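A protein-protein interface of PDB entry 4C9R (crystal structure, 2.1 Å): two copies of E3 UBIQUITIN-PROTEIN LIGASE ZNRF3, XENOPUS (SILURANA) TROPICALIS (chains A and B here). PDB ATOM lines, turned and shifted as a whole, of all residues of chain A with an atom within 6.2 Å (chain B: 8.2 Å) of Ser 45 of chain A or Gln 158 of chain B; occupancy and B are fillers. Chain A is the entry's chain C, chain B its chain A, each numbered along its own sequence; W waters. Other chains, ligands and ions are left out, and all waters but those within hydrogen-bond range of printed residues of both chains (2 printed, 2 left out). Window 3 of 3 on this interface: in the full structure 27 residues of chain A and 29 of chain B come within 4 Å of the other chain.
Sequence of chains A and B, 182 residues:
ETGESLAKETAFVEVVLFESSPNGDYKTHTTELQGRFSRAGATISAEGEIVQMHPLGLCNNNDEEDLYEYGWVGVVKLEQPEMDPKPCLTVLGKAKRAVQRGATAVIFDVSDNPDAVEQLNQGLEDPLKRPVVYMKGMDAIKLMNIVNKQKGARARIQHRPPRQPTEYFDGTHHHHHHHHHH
The backbone NH of Gln 158 of chain B is in hydrogen-bond range of the backbone carbonyl oxygen of Phe 12 of chain B (2.9 Å). The side-chain carboxylate (OE2) of Glu 14 of chain B lies within salt-bridge range of the guanidinium group (NH1) of Arg 156 of chain B (3.0 Å). The side-chain hydroxyl (OG) of Ser 45 of chain B is in hydrogen-bond range of the side-chain amide nitrogen (NE2) of Gln 158 of chain B, at 3.3 Å. N of His 159 of chain B lies within hydrogen-bond range of OG of Ser 45 of chain B, at 2.9 Å. O of Ala 46 of chain B lies within hydrogen-bond range of N of Ile 157 of chain B (2.7 Å). OE2 of Glu 47 of chain B is in salt-bridge range of NE of Arg 156 of chain B (3.0 Å).
The side-chain amide oxygen (OE1) of Gln 158 of chain A lies close to the backbone carbonyl oxygen (O) of Ser 45 of chain B (3.3 Å). The side-chain carboxylate of Glu 47 of chain B lies within hydrogen-bond range of the backbone NH of Glu 47 of chain A (2.9 Å). The guanidinium group of Arg 130 of chain A lies within salt-bridge range of the side-chain carboxylate of Glu 47 of chain B, 3.9 Å away. NE2 of Gln 158 of chain B sits close to N of Ser 45 of chain A (3.4 Å).
Of chain B, only Ser 45 (3.5 Å) and Gln 158 (3.4 Å) come within 4 Å of Ser 45 of chain A. Ala 46 of chain A touches one residue of chain B. Of the printed residues of chain B, Arg 130 of chain A touches Glu 47 and Arg 156. Of the printed residues of chain B, Gln 158 of chain A touches Ser 45 (3.3 Å). Printed residues of chain A within 4 Å of Ser 45 of chain B: Ser 45 and Gln 158. Of the printed residues of chain A, Glu 47 of chain B touches Ala 46, Glu 47 and Arg 130. The nearest residue of chain B that does not touch Ser 45 of chain A is Glu 47 of chain B (4.7 Å). The nearest residue of chain A that does not touch Gln 158 of chain B is Ile 44 of chain A (4.04 Å). The nearest printed residue of chain A that does not touch Glu 47 of chain B is Ser 45 of chain A (4.7 Å).
Water W2 lies within hydrogen-bond range of the backbone carbonyl oxygen of Ser 45 of chain A (2.8 Å), the guanidinium group of Arg 130 of chain A (3.0 Å) and the side-chain carboxylate of Glu 47 of chain B (3.3 Å). Water W1 lies within hydrogen-bond range of the guanidinium group of Arg 130 of chain A and the side-chain carboxylate of Glu 14 of chain B.
Ser 45 of chain B touches its own counterpart, Ser 45 of chain A. Ser 45 of chain A touches Gln 158 of chain B, and with the chains exchanged Gln 158 of chain A touches Ser 45 of chain B. Ala 46 of chain A touches Glu 47 of chain B, and with the chains exchanged Glu 47 of chain A touches Ala 46 of chain B. Glu 47 of chain B touches its own counterpart, Glu 47 of chain A. Of the 8 pairs that touch across the chains among the printed residues, 6 have their exchanged pair printed and touching as well.
Among the printed residues, merely in contact across the chains: Ser 45 of chain A with Ser 45 of chain B, Ala 46 of chain A with Glu 47 of chain B, Glu 47 of chain A with Ala 46 of chain B and Arg 130 of chain A with Arg 156 of chain B.
Of the 12 printed residues of chain A, 5 touch a printed residue of chain B. Hydrophobic or aromatic side chains of chain A that line the printed part of chain B: Ala 46. Along chain A the printed residues that touch a printed residue of chain B span positions 45 to 158. Hydrophobic or aromatic side chains of chain B that line the printed part of chain A: Ala 46. Along chain B the printed residues that touch a printed residue of chain A span positions 45 to 158.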
ATOM      1  N   PHE A  37      38.973  -7.269  -4.661  1.00  0.00           N
ATOM      2  CA  PHE A  37      38.106  -8.014  -3.763  1.00  0.00           C
ATOM      3  C   PHE A  37      38.761  -8.203  -2.396  1.00  0.00           C
ATOM      4  O   PHE A  37      39.789  -8.868  -2.281  1.00  0.00           O
ATOM      5  CB  PHE A  37      37.839  -9.371  -4.338  1.00  0.00           C
ATOM      6  CG  PHE A  37      36.950  -9.369  -5.560  1.00  0.00           C
ATOM      7  CD1 PHE A  37      35.579  -9.224  -5.441  1.00  0.00           C
ATOM      8  CD2 PHE A  37      37.481  -9.578  -6.826  1.00  0.00           C
ATOM      9  CE1 PHE A  37      34.754  -9.254  -6.562  1.00  0.00           C
ATOM     10  CE2 PHE A  37      36.656  -9.598  -7.949  1.00  0.00           C
ATOM     11  CZ  PHE A  37      35.293  -9.432  -7.810  1.00  0.00           C
ATOM     12  N   THR A  43      34.493 -13.421  -3.428  1.00  0.00           N
ATOM     13  CA  THR A  43      35.068 -13.042  -4.699  1.00  0.00           C
ATOM     14  C   THR A  43      34.132 -13.586  -5.753  1.00  0.00           C
ATOM     15  O   THR A  43      34.195 -14.765  -6.102  1.00  0.00           O
ATOM     16  CB  THR A  43      36.455 -13.675  -4.852  1.00  0.00           C
ATOM     17  OG1 THR A  43      37.203 -13.357  -3.699  1.00  0.00           O
ATOM     18  CG2 THR A  43      37.163 -13.158  -6.074  1.00  0.00           C
ATOM     19  N   ILE A  44      33.178 -12.757  -6.160  1.00  0.00           N
ATOM     20  CA  ILE A  44      32.246 -13.109  -7.215  1.00  0.00           C
ATOM     21  C   ILE A  44      31.749 -11.853  -7.883  1.00  0.00           C
ATOM     22  O   ILE A  44      31.886 -10.749  -7.339  1.00  0.00           O
ATOM     23  CB  ILE A  44      30.980 -13.767  -6.711  1.00  0.00           C
ATOM     24  CG1 ILE A  44      30.327 -12.925  -5.618  1.00  0.00           C
ATOM     25  CG2 ILE A  44      31.216 -15.216  -6.296  1.00  0.00           C
ATOM     26  CD1 ILE A  44      28.958 -13.462  -5.289  1.00  0.00           C
ATOM     27  N   SER A  45      31.097 -12.051  -9.019  1.00  0.00           N
ATOM     28  CA  SER A  45      30.554 -10.973  -9.785  1.00  0.00           C
ATOM     29  C   SER A  45      29.246 -10.549  -9.136  1.00  0.00           C
ATOM     30  O   SER A  45      28.577 -11.353  -8.511  1.00  0.00           O
ATOM     31  CB  SER A  45      30.340 -11.433 -11.231  1.00  0.00           C
ATOM     32  OG  SER A  45      31.589 -11.616 -11.893  1.00  0.00           O
ATOM     33  N   ALA A  46      28.909  -9.273  -9.275  1.00  0.00           N
ATOM     34  CA  ALA A  46      27.663  -8.731  -8.780  1.00  0.00           C
ATOM     35  C   ALA A  46      27.357  -7.546  -9.649  1.00  0.00           C
ATOM     36  O   ALA A  46      28.266  -6.930 -10.210  1.00  0.00           O
ATOM     37  CB  ALA A  46      27.838  -8.257  -7.335  1.00  0.00           C
ATOM     38  N   GLU A  47      26.095  -7.161  -9.702  1.00  0.00           N
ATOM     39  CA  GLU A  47      25.708  -6.024 -10.507  1.00  0.00           C
ATOM     40  C   GLU A  47      24.456  -5.398  -9.965  1.00  0.00           C
ATOM     41  O   GLU A  47      23.558  -6.090  -9.455  1.00  0.00           O
ATOM     42  CB  GLU A  47      25.567  -6.475 -11.970  1.00  0.00           C
ATOM     43  CG  GLU A  47      24.615  -5.658 -12.805  1.00  0.00           C
ATOM     44  CD  GLU A  47      24.424  -6.212 -14.221  1.00  0.00           C
ATOM     45  OE1 GLU A  47      24.880  -7.343 -14.558  1.00  0.00           O
ATOM     46  OE2 GLU A  47      23.782  -5.496 -15.005  1.00  0.00           O
ATOM     47  N   ARG A 130      28.342 -11.388  -0.246  1.00  0.00           N
ATOM     48  CA  ARG A 130      28.428 -10.456  -1.347  1.00  0.00           C
ATOM     49  C   ARG A 130      29.844  -9.892  -1.397  1.00  0.00           C
ATOM     50  O   ARG A 130      30.532  -9.889  -0.370  1.00  0.00           O
ATOM     51  CB  ARG A 130      27.405  -9.344  -1.121  1.00  0.00           C
ATOM     52  CG  ARG A 130      25.968  -9.809  -0.870  1.00  0.00           C
ATOM     53  CD  ARG A 130      25.466 -10.843  -1.869  1.00  0.00           C
ATOM     54  NE  ARG A 130      25.724 -10.389  -3.232  1.00  0.00           N
ATOM     55  CZ  ARG A 130      25.841 -11.177  -4.298  1.00  0.00           C
ATOM     56  NH1 ARG A 130      25.682 -12.485  -4.195  1.00  0.00           N
ATOM     57  NH2 ARG A 130      26.058 -10.653  -5.495  1.00  0.00           N
ATOM     58  N   PRO A 131      30.299  -9.426  -2.583  1.00  0.00           N
ATOM     59  CA  PRO A 131      31.573  -8.792  -2.690  1.00  0.00           C
ATOM     60  C   PRO A 131      31.701  -7.457  -1.981  1.00  0.00           C
ATOM     61  O   PRO A 131      30.789  -6.621  -2.011  1.00  0.00           O
ATOM     62  CB  PRO A 131      31.742  -8.601  -4.198  1.00  0.00           C
ATOM     63  CG  PRO A 131      30.412  -8.730  -4.791  1.00  0.00           C
ATOM     64  CD  PRO A 131      29.670  -9.625  -3.907  1.00  0.00           C
ATOM     65  N   ILE A 157      30.412  -5.528 -11.442  1.00  0.00           N
ATOM     66  CA  ILE A 157      31.658  -5.990 -10.814  1.00  0.00           C
ATOM     67  C   ILE A 157      31.924  -7.406 -11.305  1.00  0.00           C
ATOM     68  O   ILE A 157      31.071  -8.287 -11.130  1.00  0.00           O
ATOM     69  CB  ILE A 157      31.553  -5.960  -9.286  1.00  0.00           C
ATOM     70  CG1 ILE A 157      31.090  -4.569  -8.827  1.00  0.00           C
ATOM     71  CG2 ILE A 157      32.893  -6.331  -8.649  1.00  0.00           C
ATOM     72  CD1 ILE A 157      30.676  -4.485  -7.360  1.00  0.00           C
ATOM     73  N   GLN A 158      33.043  -7.578 -12.008  1.00  0.00           N
ATOM     74  CA  GLN A 158      33.384  -8.856 -12.611  1.00  0.00           C
ATOM     75  C   GLN A 158      34.649  -9.448 -11.979  1.00  0.00           C
ATOM     76  O   GLN A 158      35.643  -8.763 -11.761  1.00  0.00           O
ATOM     77  CB  GLN A 158      33.578  -8.759 -14.126  1.00  0.00           C
ATOM     78  CG  GLN A 158      32.372  -8.218 -14.906  1.00  0.00           C
ATOM     79  CD  GLN A 158      31.202  -9.186 -15.093  1.00  0.00           C
ATOM     80  OE1 GLN A 158      30.078  -8.752 -15.342  1.00  0.00           O
ATOM     81  NE2 GLN A 158      31.455 -10.489 -15.005  1.00  0.00           N
ATOM     82  N   HIS A 159      34.540 -10.706 -11.606  1.00  0.00           N
ATOM     83  CA  HIS A 159      35.669 -11.516 -11.295  1.00  0.00           C
ATOM     84  C   HIS A 159      36.044 -12.316 -12.553  1.00  0.00           C
ATOM     85  O   HIS A 159      35.258 -13.135 -13.021  1.00  0.00           O
ATOM     86  CB  HIS A 159      35.282 -12.466 -10.165  1.00  0.00           C
ATOM     87  CG  HIS A 159      36.343 -13.467  -9.826  1.00  0.00           C
ATOM     88  ND1 HIS A 159      36.099 -14.822  -9.786  1.00  0.00           N
ATOM     89  CD2 HIS A 159      37.648 -13.310  -9.498  1.00  0.00           C
ATOM     90  CE1 HIS A 159      37.208 -15.461  -9.452  1.00  0.00           C
ATOM     91  NE2 HIS A 159      38.169 -14.567  -9.286  1.00  0.00           N
ATOM     92  N   ARG A 160      37.227 -12.078 -13.092  1.00  0.00           N
ATOM     93  CA  ARG A 160      37.756 -12.889 -14.205  1.00  0.00           C
ATOM     94  C   ARG A 160      39.128 -13.432 -13.794  1.00  0.00           C
ATOM     95  O   ARG A 160      40.136 -12.717 -13.886  1.00  0.00           O
ATOM     96  CB  ARG A 160      37.892 -12.071 -15.495  1.00  0.00           C
ATOM     97  CG  ARG A 160      37.270 -10.682 -15.450  1.00  0.00           C
ATOM     98  CD  ARG A 160      36.616 -10.323 -16.769  1.00  0.00           C
ATOM     99  NE  ARG A 160      36.638  -8.880 -17.024  1.00  0.00           N
ATOM    100  CZ  ARG A 160      37.720  -8.194 -17.381  1.00  0.00           C
ATOM    101  NH1 ARG A 160      38.894  -8.810 -17.504  1.00  0.00           N
ATOM    102  NH2 ARG A 160      37.634  -6.883 -17.598  1.00  0.00           N
ATOM    103  N   GLU B   9      28.862 -23.774 -21.877  1.00  0.00           N
ATOM    104  CA  GLU B   9      29.105 -23.648 -20.435  1.00  0.00           C
ATOM    105  C   GLU B   9      27.826 -23.482 -19.594  1.00  0.00           C
ATOM    106  O   GLU B   9      26.827 -22.876 -20.034  1.00  0.00           O
ATOM    107  CB  GLU B   9      30.083 -22.503 -20.145  1.00  0.00           C
ATOM    108  CG  GLU B   9      31.281 -22.529 -21.089  1.00  0.00           C
ATOM    109  CD  GLU B   9      32.442 -21.706 -20.615  1.00  0.00           C
ATOM    110  OE1 GLU B   9      32.779 -21.785 -19.405  1.00  0.00           O
ATOM    111  OE2 GLU B   9      33.018 -20.987 -21.468  1.00  0.00           O
ATOM    112  N   THR B  10      27.889 -24.019 -18.380  1.00  0.00           N
ATOM    113  CA  THR B  10      26.768 -23.953 -17.449  1.00  0.00           C
ATOM    114  C   THR B  10      26.598 -22.554 -16.862  1.00  0.00           C
ATOM    115  O   THR B  10      27.593 -21.874 -16.530  1.00  0.00           O
ATOM    116  CB  THR B  10      26.903 -25.015 -16.350  1.00  0.00           C
ATOM    117  OG1 THR B  10      26.861 -26.278 -16.986  1.00  0.00           O
ATOM    118  CG2 THR B  10      25.754 -24.933 -15.354  1.00  0.00           C
ATOM    119  N   ALA B  11      25.340 -22.090 -16.874  1.00  0.00           N
ATOM    120  CA  ALA B  11      24.980 -20.818 -16.272  1.00  0.00           C
ATOM    121  C   ALA B  11      24.322 -21.144 -14.966  1.00  0.00           C
ATOM    122  O   ALA B  11      23.272 -21.802 -14.949  1.00  0.00           O
ATOM    123  CB  ALA B  11      24.022 -20.041 -17.166  1.00  0.00           C
ATOM    124  N   PHE B  12      24.947 -20.721 -13.873  1.00  0.00           N
ATOM    125  CA  PHE B  12      24.442 -21.059 -12.554  1.00  0.00           C
ATOM    126  C   PHE B  12      23.611 -19.893 -12.174  1.00  0.00           C
ATOM    127  O   PHE B  12      24.144 -18.806 -11.983  1.00  0.00           O
ATOM    128  CB  PHE B  12      25.615 -21.200 -11.570  1.00  0.00           C
ATOM    129  CG  PHE B  12      26.479 -22.393 -11.840  1.00  0.00           C
ATOM    130  CD1 PHE B  12      26.190 -23.609 -11.249  1.00  0.00           C
ATOM    131  CD2 PHE B  12      27.569 -22.304 -12.689  1.00  0.00           C
ATOM    132  CE1 PHE B  12      26.991 -24.709 -11.475  1.00  0.00           C
ATOM    133  CE2 PHE B  12      28.385 -23.404 -12.922  1.00  0.00           C
ATOM    134  CZ  PHE B  12      28.083 -24.621 -12.325  1.00  0.00           C
ATOM    135  N   VAL B  13      22.302 -20.081 -12.137  1.00  0.00           N
ATOM    136  CA  VAL B  13      21.410 -18.938 -11.972  1.00  0.00           C
ATOM    137  C   VAL B  13      20.806 -19.023 -10.588  1.00  0.00           C
ATOM    138  O   VAL B  13      20.100 -19.974 -10.268  1.00  0.00           O
ATOM    139  CB  VAL B  13      20.262 -18.921 -13.001  1.00  0.00           C
ATOM    140  CG1 VAL B  13      19.383 -17.713 -12.750  1.00  0.00           C
ATOM    141  CG2 VAL B  13      20.783 -19.007 -14.436  1.00  0.00           C
ATOM    142  N   GLU B  14      21.097 -18.022  -9.784  1.00  0.00           N
ATOM    143  CA  GLU B  14      20.555 -17.939  -8.445  1.00  0.00           C
ATOM    144  C   GLU B  14      19.405 -16.963  -8.502  1.00  0.00           C
ATOM    145  O   GLU B  14      19.546 -15.872  -9.040  1.00  0.00           O
ATOM    146  CB  GLU B  14      21.686 -17.579  -7.466  1.00  0.00           C
ATOM    147  CG  GLU B  14      21.267 -16.813  -6.231  1.00  0.00           C
ATOM    148  CD  GLU B  14      22.472 -16.294  -5.425  1.00  0.00           C
ATOM    149  OE1 GLU B  14      23.568 -16.870  -5.594  1.00  0.00           O
ATOM    150  OE2 GLU B  14      22.333 -15.312  -4.633  1.00  0.00           O
ATOM    151  N   LEU B  33      19.458 -22.536  -9.802  1.00  0.00           N
ATOM    152  CA  LEU B  33      19.036 -23.146 -11.043  1.00  0.00           C
ATOM    153  C   LEU B  33      20.234 -23.242 -11.960  1.00  0.00           C
ATOM    154  O   LEU B  33      21.246 -22.614 -11.748  1.00  0.00           O
ATOM    155  CB  LEU B  33      17.917 -22.305 -11.727  1.00  0.00           C
ATOM    156  CG  LEU B  33      16.678 -21.901 -10.890  1.00  0.00           C
ATOM    157  CD1 LEU B  33      15.657 -21.050 -11.627  1.00  0.00           C
ATOM    158  CD2 LEU B  33      15.957 -23.142 -10.387  1.00  0.00           C
ATOM    159  N   GLY B  35      21.218 -23.321 -16.227  1.00  0.00           N
ATOM    160  CA  GLY B  35      20.975 -23.383 -17.660  1.00  0.00           C
ATOM    161  C   GLY B  35      22.309 -23.420 -18.330  1.00  0.00           C
ATOM    162  O   GLY B  35      23.290 -23.830 -17.739  1.00  0.00           O
ATOM    163  N   PHE B  37      24.955 -21.048 -21.128  1.00  0.00           N
ATOM    164  CA  PHE B  37      25.224 -19.861 -21.898  1.00  0.00           C
ATOM    165  C   PHE B  37      25.172 -20.206 -23.398  1.00  0.00           C
ATOM    166  O   PHE B  37      25.904 -21.116 -23.875  1.00  0.00           O
ATOM    167  CB  PHE B  37      26.614 -19.300 -21.583  1.00  0.00           C
ATOM    168  CG  PHE B  37      26.737 -18.661 -20.227  1.00  0.00           C
ATOM    169  CD1 PHE B  37      26.276 -17.383 -20.013  1.00  0.00           C
ATOM    170  CD2 PHE B  37      27.366 -19.330 -19.180  1.00  0.00           C
ATOM    171  CE1 PHE B  37      26.368 -16.793 -18.762  1.00  0.00           C
ATOM    172  CE2 PHE B  37      27.457 -18.763 -17.929  1.00  0.00           C
ATOM    173  CZ  PHE B  37      26.956 -17.487 -17.712  1.00  0.00           C
ATOM    174  N   THR B  43      29.556 -15.059 -22.652  1.00  0.00           N
ATOM    175  CA  THR B  43      29.616 -15.950 -21.479  1.00  0.00           C
ATOM    176  C   THR B  43      30.151 -15.136 -20.280  1.00  0.00           C
ATOM    177  O   THR B  43      31.333 -15.149 -19.986  1.00  0.00           O
ATOM    178  CB  THR B  43      30.428 -17.197 -21.816  1.00  0.00           C
ATOM    179  OG1 THR B  43      29.680 -17.955 -22.790  1.00  0.00           O
ATOM    180  CG2 THR B  43      30.701 -18.112 -20.575  1.00  0.00           C
ATOM    181  N   ILE B  44      29.251 -14.383 -19.640  1.00  0.00           N
ATOM    182  CA  ILE B  44      29.572 -13.599 -18.458  1.00  0.00           C
ATOM    183  C   ILE B  44      28.428 -13.583 -17.451  1.00  0.00           C
ATOM    184  O   ILE B  44      27.297 -13.931 -17.768  1.00  0.00           O
ATOM    185  CB  ILE B  44      29.815 -12.123 -18.811  1.00  0.00           C
ATOM    186  CG1 ILE B  44      28.648 -11.568 -19.656  1.00  0.00           C
ATOM    187  CG2 ILE B  44      31.128 -11.970 -19.557  1.00  0.00           C
ATOM    188  CD1 ILE B  44      28.624 -10.058 -19.728  1.00  0.00           C
ATOM    189  N   SER B  45      28.774 -13.212 -16.231  1.00  0.00           N
ATOM    190  CA  SER B  45      27.859 -13.044 -15.161  1.00  0.00           C
ATOM    191  C   SER B  45      27.101 -11.771 -15.374  1.00  0.00           C
ATOM    192  O   SER B  45      27.624 -10.816 -15.945  1.00  0.00           O
ATOM    193  CB  SER B  45      28.624 -12.963 -13.838  1.00  0.00           C
ATOM    194  OG  SER B  45      29.311 -14.165 -13.597  1.00  0.00           O
ATOM    195  N   ALA B  46      25.855 -11.760 -14.915  1.00  0.00           N
ATOM    196  CA  ALA B  46      24.944 -10.611 -15.033  1.00  0.00           C
ATOM    197  C   ALA B  46      23.944 -10.786 -13.932  1.00  0.00           C
ATOM    198  O   ALA B  46      23.637 -11.922 -13.531  1.00  0.00           O
ATOM    199  CB  ALA B  46      24.196 -10.662 -16.362  1.00  0.00           C
ATOM    200  N   GLU B  47      23.362  -9.687 -13.513  1.00  0.00           N
ATOM    201  CA  GLU B  47      22.408  -9.684 -12.420  1.00  0.00           C
ATOM    202  C   GLU B  47      21.434  -8.549 -12.583  1.00  0.00           C
ATOM    203  O   GLU B  47      21.801  -7.432 -12.995  1.00  0.00           O
ATOM    204  CB  GLU B  47      23.167  -9.611 -11.091  1.00  0.00           C
ATOM    205  CG  GLU B  47      22.345  -9.077  -9.947  1.00  0.00           C
ATOM    206  CD  GLU B  47      23.129  -9.034  -8.623  1.00  0.00           C
ATOM    207  OE1 GLU B  47      24.361  -9.195  -8.630  1.00  0.00           O
ATOM    208  OE2 GLU B  47      22.483  -8.830  -7.577  1.00  0.00           O
ATOM    209  N   PRO B 131      24.711 -11.813 -21.667  1.00  0.00           N
ATOM    210  CA  PRO B 131      24.419 -13.256 -21.726  1.00  0.00           C
ATOM    211  C   PRO B 131      23.018 -13.593 -22.192  1.00  0.00           C
ATOM    212  O   PRO B 131      22.052 -12.892 -21.864  1.00  0.00           O
ATOM    213  CB  PRO B 131      24.656 -13.744 -20.305  1.00  0.00           C
ATOM    214  CG  PRO B 131      24.607 -12.525 -19.442  1.00  0.00           C
ATOM    215  CD  PRO B 131      24.956 -11.343 -20.296  1.00  0.00           C
ATOM    216  N   VAL B 133      20.886 -16.949 -22.084  1.00  0.00           N
ATOM    217  CA  VAL B 133      20.908 -18.194 -21.395  1.00  0.00           C
ATOM    218  C   VAL B 133      19.647 -18.964 -21.773  1.00  0.00           C
ATOM    219  O   VAL B 133      18.589 -18.359 -21.975  1.00  0.00           O
ATOM    220  CB  VAL B 133      21.017 -17.940 -19.862  1.00  0.00           C
ATOM    221  CG1 VAL B 133      20.703 -19.226 -19.024  1.00  0.00           C
ATOM    222  CG2 VAL B 133      22.382 -17.390 -19.519  1.00  0.00           C
ATOM    223  N   ALA B 155      17.623 -12.127 -10.424  1.00  0.00           N
ATOM    224  CA  ALA B 155      18.447 -13.187 -10.934  1.00  0.00           C
ATOM    225  C   ALA B 155      19.885 -12.761 -10.912  1.00  0.00           C
ATOM    226  O   ALA B 155      20.204 -11.652 -11.326  1.00  0.00           O
ATOM    227  CB  ALA B 155      18.047 -13.565 -12.352  1.00  0.00           C
ATOM    228  N   ARG B 156      20.728 -13.645 -10.419  1.00  0.00           N
ATOM    229  CA  ARG B 156      22.165 -13.514 -10.478  1.00  0.00           C
ATOM    230  C   ARG B 156      22.686 -14.663 -11.346  1.00  0.00           C
ATOM    231  O   ARG B 156      22.674 -15.830 -10.910  1.00  0.00           O
ATOM    232  CB  ARG B 156      22.769 -13.643  -9.086  1.00  0.00           C
ATOM    233  CG  ARG B 156      22.196 -12.617  -8.149  1.00  0.00           C
ATOM    234  CD  ARG B 156      22.804 -12.685  -6.760  1.00  0.00           C
ATOM    235  NE  ARG B 156      22.486 -11.420  -6.087  1.00  0.00           N
ATOM    236  CZ  ARG B 156      22.206 -11.307  -4.781  1.00  0.00           C
ATOM    237  NH1 ARG B 156      22.182 -12.387  -4.019  1.00  0.00           N
ATOM    238  NH2 ARG B 156      21.930 -10.120  -4.250  1.00  0.00           N
ATOM    239  N   ILE B 157      23.098 -14.335 -12.560  1.00  0.00           N
ATOM    240  CA  ILE B 157      23.600 -15.334 -13.490  1.00  0.00           C
ATOM    241  C   ILE B 157      25.112 -15.349 -13.301  1.00  0.00           C
ATOM    242  O   ILE B 157      25.753 -14.332 -13.455  1.00  0.00           O
ATOM    243  CB  ILE B 157      23.281 -14.979 -14.935  1.00  0.00           C
ATOM    244  CG1 ILE B 157      21.778 -15.045 -15.160  1.00  0.00           C
ATOM    245  CG2 ILE B 157      24.029 -15.847 -15.926  1.00  0.00           C
ATOM    246  CD1 ILE B 157      21.324 -14.223 -16.356  1.00  0.00           C
ATOM    247  N   GLN B 158      25.642 -16.500 -12.894  1.00  0.00           N
ATOM    248  CA  GLN B 158      27.051 -16.623 -12.556  1.00  0.00           C
ATOM    249  C   GLN B 158      27.762 -17.539 -13.594  1.00  0.00           C
ATOM    250  O   GLN B 158      27.322 -18.632 -13.897  1.00  0.00           O
ATOM    251  CB  GLN B 158      27.153 -17.184 -11.125  1.00  0.00           C
ATOM    252  CG  GLN B 158      28.345 -16.762 -10.268  1.00  0.00           C
ATOM    253  CD  GLN B 158      28.665 -15.259 -10.216  1.00  0.00           C
ATOM    254  OE1 GLN B 158      27.804 -14.412  -9.948  1.00  0.00           O
ATOM    255  NE2 GLN B 158      29.955 -14.934 -10.444  1.00  0.00           N
ATOM    256  N   HIS B 159      28.824 -17.015 -14.182  1.00  0.00           N
ATOM    257  CA  HIS B 159      29.748 -17.794 -14.912  1.00  0.00           C
ATOM    258  C   HIS B 159      30.760 -18.282 -13.897  1.00  0.00           C
ATOM    259  O   HIS B 159      31.537 -17.486 -13.417  1.00  0.00           O
ATOM    260  CB  HIS B 159      30.447 -16.912 -15.941  1.00  0.00           C
ATOM    261  CG  HIS B 159      31.527 -17.624 -16.696  1.00  0.00           C
ATOM    262  ND1 HIS B 159      32.697 -17.010 -17.074  1.00  0.00           N
ATOM    263  CD2 HIS B 159      31.612 -18.905 -17.135  1.00  0.00           C
ATOM    264  CE1 HIS B 159      33.466 -17.885 -17.702  1.00  0.00           C
ATOM    265  NE2 HIS B 159      32.828 -19.038 -17.762  1.00  0.00           N
ATOM    266  N   ARG B 160      30.726 -19.551 -13.513  1.00  0.00           N
ATOM    267  CA  ARG B 160      31.731 -20.071 -12.566  1.00  0.00           C
ATOM    268  C   ARG B 160      32.975 -20.541 -13.318  1.00  0.00           C
ATOM    269  O   ARG B 160      32.945 -21.596 -13.960  1.00  0.00           O
ATOM    270  CB  ARG B 160      31.190 -21.241 -11.767  1.00  0.00           C
ATOM    271  CG  ARG B 160      30.125 -20.871 -10.763  1.00  0.00           C
ATOM    272  CD  ARG B 160      30.215 -21.812  -9.586  1.00  0.00           C
ATOM    273  NE  ARG B 160      28.921 -22.215  -9.056  1.00  0.00           N
ATOM    274  CZ  ARG B 160      27.977 -21.383  -8.630  1.00  0.00           C
ATOM    275  NH1 ARG B 160      28.126 -20.061  -8.695  1.00  0.00           N
ATOM    276  NH2 ARG B 160      26.848 -21.888  -8.161  1.00  0.00           N
ATOM    277  N   PRO B 161      34.084 -19.784 -13.218  1.00  0.00           N
ATOM    278  CA  PRO B 161      35.258 -20.104 -14.022  1.00  0.00           C
ATOM    279  C   PRO B 161      36.108 -21.232 -13.403  1.00  0.00           C
ATOM    280  O   PRO B 161      35.730 -22.407 -13.465  1.00  0.00           O
ATOM    281  CB  PRO B 161      36.029 -18.784 -14.009  1.00  0.00           C
ATOM    282  CG  PRO B 161      35.726 -18.202 -12.653  1.00  0.00           C
ATOM    283  CD  PRO B 161      34.406 -18.775 -12.186  1.00  0.00           C
HETATM  284  O   HOH W   1      24.812 -14.697  -2.617  1.00  0.00           O
HETATM  285  O   HOH W   2      25.929 -12.043  -8.154  1.00  0.00           O
